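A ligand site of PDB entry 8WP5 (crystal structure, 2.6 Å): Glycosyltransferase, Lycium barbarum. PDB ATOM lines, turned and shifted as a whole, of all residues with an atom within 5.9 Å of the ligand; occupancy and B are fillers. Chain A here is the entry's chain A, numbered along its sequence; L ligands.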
ATOM      1  N   ASN A 257      -9.610  11.906   3.072  1.00  0.00           N
ATOM      2  CA  ASN A 257     -10.049  12.530   1.826  1.00  0.00           C
ATOM      3  C   ASN A 257      -9.278  11.916   0.664  1.00  0.00           C
ATOM      4  O   ASN A 257      -8.085  12.172   0.498  1.00  0.00           O
ATOM      5  CB  ASN A 257      -9.830  14.039   1.891  1.00  0.00           C
ATOM      6  CG  ASN A 257      -9.904  14.703   0.527  1.00  0.00           C
ATOM      7  OD1 ASN A 257      -8.940  15.315   0.066  1.00  0.00           O
ATOM      8  ND2 ASN A 257     -11.057  14.579  -0.128  1.00  0.00           N
ATOM      9  N   CYS A 290       8.054   8.471   1.177  1.00  0.00           N
ATOM     10  CA  CYS A 290       7.334   9.732   1.363  1.00  0.00           C
ATOM     11  C   CYS A 290       7.353  10.113   2.833  1.00  0.00           C
ATOM     12  O   CYS A 290       7.370   9.252   3.715  1.00  0.00           O
ATOM     13  CB  CYS A 290       5.889   9.635   0.862  1.00  0.00           C
ATOM     14  SG  CYS A 290       5.273  11.187   0.157  1.00  0.00           S
ATOM     15  N   PHE A 291       7.355  11.431   3.098  1.00  0.00           N
ATOM     16  CA  PHE A 291       7.572  11.938   4.452  1.00  0.00           C
ATOM     17  C   PHE A 291       6.727  13.175   4.715  1.00  0.00           C
ATOM     18  O   PHE A 291       7.215  14.163   5.294  1.00  0.00           O
ATOM     19  CB  PHE A 291       9.053  12.241   4.690  1.00  0.00           C
ATOM     20  CG  PHE A 291       9.964  11.086   4.393  1.00  0.00           C
ATOM     21  CD1 PHE A 291      10.194  10.113   5.353  1.00  0.00           C
ATOM     22  CD2 PHE A 291      10.581  10.956   3.165  1.00  0.00           C
ATOM     23  CE1 PHE A 291      11.021   9.041   5.090  1.00  0.00           C
ATOM     24  CE2 PHE A 291      11.414   9.895   2.895  1.00  0.00           C
ATOM     25  CZ  PHE A 291      11.636   8.933   3.852  1.00  0.00           C
ATOM     26  N   GLY A 292       5.471  13.157   4.316  1.00  0.00           N
ATOM     27  CA  GLY A 292       4.524  14.172   4.724  1.00  0.00           C
ATOM     28  C   GLY A 292       4.775  15.555   4.160  1.00  0.00           C
ATOM     29  O   GLY A 292       5.668  15.789   3.335  1.00  0.00           O
ATOM     30  N   SER A 293       3.969  16.505   4.647  1.00  0.00           N
ATOM     31  CA  SER A 293       3.884  17.823   4.028  1.00  0.00           C
ATOM     32  C   SER A 293       5.184  18.610   4.209  1.00  0.00           C
ATOM     33  O   SER A 293       5.628  19.297   3.280  1.00  0.00           O
ATOM     34  CB  SER A 293       2.702  18.604   4.610  1.00  0.00           C
ATOM     35  OG  SER A 293       2.706  18.589   6.020  1.00  0.00           O
ATOM     36  N   MET A 294       5.797  18.533   5.392  1.00  0.00           N
ATOM     37  CA  MET A 294       6.967  19.349   5.700  1.00  0.00           C
ATOM     38  C   MET A 294       8.228  18.513   5.911  1.00  0.00           C
ATOM     39  O   MET A 294       9.251  19.055   6.343  1.00  0.00           O
ATOM     40  CB  MET A 294       6.683  20.215   6.931  1.00  0.00           C
ATOM     41  CG  MET A 294       7.565  21.454   7.057  1.00  0.00           C
ATOM     42  SD  MET A 294       7.407  22.209   8.686  1.00  0.00           S
ATOM     43  CE  MET A 294       7.013  20.766   9.658  1.00  0.00           C
ATOM     44  N   SER A 319       9.702   9.971  -3.253  1.00  0.00           N
ATOM     45  CA  SER A 319       9.299  11.374  -3.277  1.00  0.00           C
ATOM     46  C   SER A 319      10.367  12.187  -2.555  1.00  0.00           C
ATOM     47  O   SER A 319      10.502  12.093  -1.337  1.00  0.00           O
ATOM     48  CB  SER A 319       7.929  11.557  -2.624  1.00  0.00           C
ATOM     49  OG  SER A 319       8.050  11.993  -1.286  1.00  0.00           O
ATOM     50  N   ARG A 321      11.826  15.955  -1.852  1.00  0.00           N
ATOM     51  CA  ARG A 321      11.537  17.378  -1.869  1.00  0.00           C
ATOM     52  C   ARG A 321      12.770  18.169  -1.450  1.00  0.00           C
ATOM     53  O   ARG A 321      13.664  17.650  -0.779  1.00  0.00           O
ATOM     54  CB  ARG A 321      10.355  17.713  -0.956  1.00  0.00           C
ATOM     55  CG  ARG A 321       9.167  16.771  -1.118  1.00  0.00           C
ATOM     56  CD  ARG A 321       7.841  17.481  -0.876  1.00  0.00           C
ATOM     57  NE  ARG A 321       7.714  18.757  -1.581  1.00  0.00           N
ATOM     58  CZ  ARG A 321       7.164  19.829  -1.041  1.00  0.00           C
ATOM     59  NH1 ARG A 321       6.718  19.768   0.210  1.00  0.00           N
ATOM     60  NH2 ARG A 321       7.055  20.966  -1.719  1.00  0.00           N
ATOM     61  N   GLY A 358       9.037  14.588  -6.815  1.00  0.00           N
ATOM     62  CA  GLY A 358       8.900  15.516  -5.714  1.00  0.00           C
ATOM     63  C   GLY A 358       7.639  15.227  -4.925  1.00  0.00           C
ATOM     64  O   GLY A 358       7.499  14.148  -4.341  1.00  0.00           O
ATOM     65  N   TRP A 359       6.706  16.176  -4.896  1.00  0.00           N
ATOM     66  CA  TRP A 359       5.404  15.935  -4.296  1.00  0.00           C
ATOM     67  C   TRP A 359       4.708  14.798  -5.030  1.00  0.00           C
ATOM     68  O   TRP A 359       4.792  14.682  -6.260  1.00  0.00           O
ATOM     69  CB  TRP A 359       4.558  17.203  -4.327  1.00  0.00           C
ATOM     70  CG  TRP A 359       3.175  17.059  -3.780  1.00  0.00           C
ATOM     71  CD1 TRP A 359       2.059  16.723  -4.466  1.00  0.00           C
ATOM     72  CD2 TRP A 359       2.755  17.263  -2.424  1.00  0.00           C
ATOM     73  NE1 TRP A 359       0.964  16.701  -3.644  1.00  0.00           N
ATOM     74  CE2 TRP A 359       1.364  17.024  -2.376  1.00  0.00           C
ATOM     75  CE3 TRP A 359       3.424  17.620  -1.245  1.00  0.00           C
ATOM     76  CZ2 TRP A 359       0.634  17.142  -1.199  1.00  0.00           C
ATOM     77  CZ3 TRP A 359       2.684  17.720  -0.076  1.00  0.00           C
ATOM     78  CH2 TRP A 359       1.308  17.485  -0.054  1.00  0.00           C
ATOM     79  N   ALA A 360       4.019  13.949  -4.279  1.00  0.00           N
ATOM     80  CA  ALA A 360       3.470  12.728  -4.840  1.00  0.00           C
ATOM     81  C   ALA A 360       1.973  12.612  -4.570  1.00  0.00           C
ATOM     82  O   ALA A 360       1.502  13.001  -3.492  1.00  0.00           O
ATOM     83  CB  ALA A 360       4.183  11.496  -4.258  1.00  0.00           C
ATOM     84  N   PRO A 361       1.205  12.091  -5.526  1.00  0.00           N
ATOM     85  CA  PRO A 361      -0.195  11.749  -5.233  1.00  0.00           C
ATOM     86  C   PRO A 361      -0.259  10.543  -4.314  1.00  0.00           C
ATOM     87  O   PRO A 361      -0.359   9.399  -4.770  1.00  0.00           O
ATOM     88  CB  PRO A 361      -0.780  11.442  -6.623  1.00  0.00           C
ATOM     89  CG  PRO A 361       0.392  11.019  -7.438  1.00  0.00           C
ATOM     90  CD  PRO A 361       1.566  11.819  -6.924  1.00  0.00           C
ATOM     91  N   GLN A 362      -0.188  10.805  -3.003  1.00  0.00           N
ATOM     92  CA  GLN A 362       0.029   9.738  -2.028  1.00  0.00           C
ATOM     93  C   GLN A 362      -1.072   8.680  -2.089  1.00  0.00           C
ATOM     94  O   GLN A 362      -0.786   7.470  -2.126  1.00  0.00           O
ATOM     95  CB  GLN A 362       0.122  10.329  -0.628  1.00  0.00           C
ATOM     96  CG  GLN A 362       0.532   9.332   0.439  1.00  0.00           C
ATOM     97  CD  GLN A 362       1.043  10.005   1.699  1.00  0.00           C
ATOM     98  OE1 GLN A 362       2.048  10.710   1.674  1.00  0.00           O
ATOM     99  NE2 GLN A 362       0.344   9.785   2.814  1.00  0.00           N
ATOM    100  N   VAL A 363      -2.332   9.105  -2.112  1.00  0.00           N
ATOM    101  CA  VAL A 363      -3.434   8.148  -2.115  1.00  0.00           C
ATOM    102  C   VAL A 363      -3.460   7.372  -3.423  1.00  0.00           C
ATOM    103  O   VAL A 363      -3.691   6.151  -3.434  1.00  0.00           O
ATOM    104  CB  VAL A 363      -4.777   8.877  -1.857  1.00  0.00           C
ATOM    105  CG1 VAL A 363      -5.942   8.060  -2.392  1.00  0.00           C
ATOM    106  CG2 VAL A 363      -4.934   9.138  -0.372  1.00  0.00           C
ATOM    107  N   HIS A 377       7.069   8.920   7.530  1.00  0.00           N
ATOM    108  CA  HIS A 377       7.291   9.628   8.787  1.00  0.00           C
ATOM    109  C   HIS A 377       6.230   9.310   9.818  1.00  0.00           C
ATOM    110  O   HIS A 377       6.332   9.796  10.946  1.00  0.00           O
ATOM    111  CB  HIS A 377       7.337  11.127   8.526  1.00  0.00           C
ATOM    112  CG  HIS A 377       6.021  11.701   8.092  1.00  0.00           C
ATOM    113  ND1 HIS A 377       5.608  12.969   8.434  1.00  0.00           N
ATOM    114  CD2 HIS A 377       5.019  11.173   7.340  1.00  0.00           C
ATOM    115  CE1 HIS A 377       4.412  13.201   7.917  1.00  0.00           C
ATOM    116  NE2 HIS A 377       4.034  12.117   7.248  1.00  0.00           N
ATOM    117  N   CYS A 378       5.216   8.521   9.461  1.00  0.00           N
ATOM    118  CA  CYS A 378       4.163   8.062  10.363  1.00  0.00           C
ATOM    119  C   CYS A 378       3.270   9.204  10.840  1.00  0.00           C
ATOM    120  O   CYS A 378       2.729   9.156  11.949  1.00  0.00           O
ATOM    121  CB  CYS A 378       4.744   7.304  11.555  1.00  0.00           C
ATOM    122  SG  CYS A 378       5.799   5.911  11.098  1.00  0.00           S
ATOM    123  N   GLY A 379       3.101  10.238  10.024  1.00  0.00           N
ATOM    124  CA  GLY A 379       1.986  11.140  10.234  1.00  0.00           C
ATOM    125  C   GLY A 379       0.674  10.382  10.132  1.00  0.00           C
ATOM    126  O   GLY A 379       0.499   9.531   9.260  1.00  0.00           O
ATOM    127  N   TRP A 380      -0.250  10.685  11.043  1.00  0.00           N
ATOM    128  CA  TRP A 380      -1.379   9.777  11.239  1.00  0.00           C
ATOM    129  C   TRP A 380      -2.287   9.711  10.025  1.00  0.00           C
ATOM    130  O   TRP A 380      -2.819   8.641   9.699  1.00  0.00           O
ATOM    131  CB  TRP A 380      -2.184  10.176  12.480  1.00  0.00           C
ATOM    132  CG  TRP A 380      -3.173   9.106  12.833  1.00  0.00           C
ATOM    133  CD1 TRP A 380      -4.528   9.223  12.867  1.00  0.00           C
ATOM    134  CD2 TRP A 380      -2.880   7.732  13.145  1.00  0.00           C
ATOM    135  NE1 TRP A 380      -5.101   8.019  13.211  1.00  0.00           N
ATOM    136  CE2 TRP A 380      -4.107   7.091  13.378  1.00  0.00           C
ATOM    137  CE3 TRP A 380      -1.702   7.001  13.266  1.00  0.00           C
ATOM    138  CZ2 TRP A 380      -4.195   5.743  13.727  1.00  0.00           C
ATOM    139  CZ3 TRP A 380      -1.784   5.664  13.608  1.00  0.00           C
ATOM    140  CH2 TRP A 380      -3.018   5.053  13.842  1.00  0.00           C
ATOM    141  N   ASN A 381      -2.500  10.831   9.322  1.00  0.00           N
ATOM    142  CA  ASN A 381      -3.254  10.777   8.079  1.00  0.00           C
ATOM    143  C   ASN A 381      -2.584   9.859   7.075  1.00  0.00           C
ATOM    144  O   ASN A 381      -3.255   9.068   6.388  1.00  0.00           O
ATOM    145  CB  ASN A 381      -3.432  12.179   7.491  1.00  0.00           C
ATOM    146  CG  ASN A 381      -4.543  12.960   8.157  1.00  0.00           C
ATOM    147  OD1 ASN A 381      -5.674  12.482   8.281  1.00  0.00           O
ATOM    148  ND2 ASN A 381      -4.233  14.186   8.566  1.00  0.00           N
ATOM    149  N   SER A 382      -1.251   9.938   6.975  1.00  0.00           N
ATOM    150  CA  SER A 382      -0.525   9.058   6.074  1.00  0.00           C
ATOM    151  C   SER A 382      -0.673   7.593   6.478  1.00  0.00           C
ATOM    152  O   SER A 382      -0.765   6.714   5.614  1.00  0.00           O
ATOM    153  CB  SER A 382       0.956   9.460   6.039  1.00  0.00           C
ATOM    154  OG  SER A 382       1.168  10.579   5.200  1.00  0.00           O
ATOM    155  N   GLU A 385      -4.085   6.300   5.494  1.00  0.00           N
ATOM    156  CA  GLU A 385      -4.128   6.068   4.054  1.00  0.00           C
ATOM    157  C   GLU A 385      -3.407   4.780   3.681  1.00  0.00           C
ATOM    158  O   GLU A 385      -3.884   4.022   2.830  1.00  0.00           O
ATOM    159  CB  GLU A 385      -3.522   7.259   3.313  1.00  0.00           C
ATOM    160  CG  GLU A 385      -4.389   8.499   3.336  1.00  0.00           C
ATOM    161  CD  GLU A 385      -3.618   9.757   3.004  1.00  0.00           C
ATOM    162  OE1 GLU A 385      -4.246  10.843   2.976  1.00  0.00           O
ATOM    163  OE2 GLU A 385      -2.399   9.677   2.762  1.00  0.00           O
ATOM    164  N   TYR A 399       8.719  14.550  13.245  1.00  0.00           N
ATOM    165  CA  TYR A 399       8.329  15.627  14.137  1.00  0.00           C
ATOM    166  C   TYR A 399       6.946  15.334  14.721  1.00  0.00           C
ATOM    167  O   TYR A 399       6.324  14.310  14.409  1.00  0.00           O
ATOM    168  CB  TYR A 399       8.330  16.978  13.409  1.00  0.00           C
ATOM    169  CG  TYR A 399       7.558  16.967  12.105  1.00  0.00           C
ATOM    170  CD1 TYR A 399       6.190  17.186  12.088  1.00  0.00           C
ATOM    171  CD2 TYR A 399       8.199  16.751  10.890  1.00  0.00           C
ATOM    172  CE1 TYR A 399       5.475  17.181  10.896  1.00  0.00           C
ATOM    173  CE2 TYR A 399       7.507  16.744   9.698  1.00  0.00           C
ATOM    174  CZ  TYR A 399       6.138  16.959   9.703  1.00  0.00           C
ATOM    175  OH  TYR A 399       5.437  16.960   8.531  1.00  0.00           O
ATOM    176  N   GLN A 402       4.906  11.858  15.757  1.00  0.00           N
ATOM    177  CA  GLN A 402       5.181  10.751  14.856  1.00  0.00           C
ATOM    178  C   GLN A 402       6.064   9.688  15.496  1.00  0.00           C
ATOM    179  O   GLN A 402       5.977   8.506  15.133  1.00  0.00           O
ATOM    180  CB  GLN A 402       5.820  11.271  13.565  1.00  0.00           C
ATOM    181  CG  GLN A 402       4.848  12.047  12.690  1.00  0.00           C
ATOM    182  CD  GLN A 402       5.547  12.958  11.700  1.00  0.00           C
ATOM    183  OE1 GLN A 402       4.904  13.720  10.980  1.00  0.00           O
ATOM    184  NE2 GLN A 402       6.870  12.876  11.653  1.00  0.00           N
HETATM  185  N1  LIG L   1       0.885  14.186   1.003  1.00  0.00           N
HETATM  186  C1  LIG L   1       0.902  14.039  -0.371  1.00  0.00           C
HETATM  187  N2  LIG L   1       2.155  13.983  -0.933  1.00  0.00           N
HETATM  188  C2  LIG L   1       3.370  14.049  -0.264  1.00  0.00           C
HETATM  189  C3  LIG L   1       3.258  14.194   1.161  1.00  0.00           C
HETATM  190  C4  LIG L   1       2.053  14.253   1.740  1.00  0.00           C
HETATM  191  O1  LIG L   1      -0.115  13.969  -1.048  1.00  0.00           O
HETATM  192  O2  LIG L   1       4.428  13.993  -0.910  1.00  0.00           O
HETATM  193  C5  LIG L   1      -0.425  14.238   1.672  1.00  0.00           C
HETATM  194  C6  LIG L   1      -0.925  12.871   2.149  1.00  0.00           C
HETATM  195  O3  LIG L   1      -1.795  12.320   1.180  1.00  0.00           O
HETATM  196  C7  LIG L   1      -1.673  13.216   3.438  1.00  0.00           C
HETATM  197  C8  LIG L   1      -0.951  14.459   3.959  1.00  0.00           C
HETATM  198  O4  LIG L   1      -0.307  15.065   2.819  1.00  0.00           O
HETATM  199  O5  LIG L   1      -3.055  13.439   3.230  1.00  0.00           O
HETATM  200  C9  LIG L   1       0.072  14.213   5.045  1.00  0.00           C
HETATM  201  O6  LIG L   1      -0.574  13.635   6.199  1.00  0.00           O
HETATM  202  P1  LIG L   1       0.104  13.683   7.629  1.00  0.00           P
HETATM  203  O7  LIG L   1       1.402  12.994   7.512  1.00  0.00           O
HETATM  204  O8  LIG L   1      -0.843  13.184   8.710  1.00  0.00           O
HETATM  205  O9  LIG L   1       0.325  15.246   7.908  1.00  0.00           O
HETATM  206  P2  LIG L   1       1.705  15.953   8.213  1.00  0.00           P
HETATM  207  O10 LIG L   1       2.417  14.930   9.109  1.00  0.00           O
HETATM  208  O11 LIG L   1       2.365  16.027   6.840  1.00  0.00           O
HETATM  209  O12 LIG L   1       1.525  17.278   8.873  1.00  0.00           O
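Merely in contact with the ligand: Gly 292 (3.5 Å), Trp 359 (3.2 Å), Gln 362 (3.3 Å), Gly 379 (3.3 Å) and Tyr 399 (3.6 Å).
Hydrophobic or aromatic side chains within 4 Å of the ligand: Trp 359 and His 377.
Of the 23 residues printed, 14 come within 4 Å of the ligand.
Along chain A the residues within 4 Å of the ligand span positions 290 to 402.
The nearest printed residue that does not touch the ligand is Ser 319 (4.2 Å).
OE1 of Gln 362 lies within hydrogen-bond range of SG of Cys 290, 3.6 Å away.
N of Tyr 399 sits close to NE2 of Gln 402, 3.0 Å away.
OE2 of Glu 385 lies within hydrogen-bond range of NE2 of Gln 362 (2.7 Å).
The side-chain hydroxyl of Ser 319 is in hydrogen-bond range of the side-chain sulfur of Cys 290 (3.2 Å).
The backbone carbonyl oxygen (O) of Ser 293 sits at hydrogen-bond distance from the guanidinium group (NH1) of Arg 321 (3.3 Å).
NE2 of His 377 sits close to N of Gly 379 (3.5 Å).
NE2 of His 377 lies close to N of Gly 292, 3.4 Å away.
OG of Ser 382 is in hydrogen-bond range of NE2 of Gln 362, 2.6 Å away.
An oxygen (O10) of the ligand sits close to the side-chain amide oxygen of Gln 402.
O7 of the ligand lies within hydrogen-bond range of NE2 of His 377 (2.8 Å).
An oxygen (O8) of the ligand lies within hydrogen-bond range of the backbone NH (N) of Asn 381 (2.9 Å).
The side-chain hydroxyl of Ser 293 lies within hydrogen-bond range of an oxygen (O11) of the ligand, at 2.7 Å.
The backbone NH of Ala 360 lies within hydrogen-bond range of an oxygen (O2) of the ligand.
SG of Cys 290 is in hydrogen-bond range of O2 of the ligand (3.1 Å).
The backbone NH (N) of Ser 293 is in hydrogen-bond range of an oxygen (O11) of the ligand (2.8 Å).
The backbone carbonyl oxygen (O) of Ala 360 lies within hydrogen-bond range of a nitrogen (N2) of the ligand, 2.8 Å away.
An oxygen (O5) of the ligand sits at hydrogen-bond distance from the side-chain carboxylate (OE1) of Glu 385, at 2.9 Å.
An oxygen (O7) of the ligand lies within hydrogen-bond range of the side-chain hydroxyl (OG) of Ser 382.
N of Trp 380 is in hydrogen-bond range of O8 of the ligand, 3.5 Å away.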
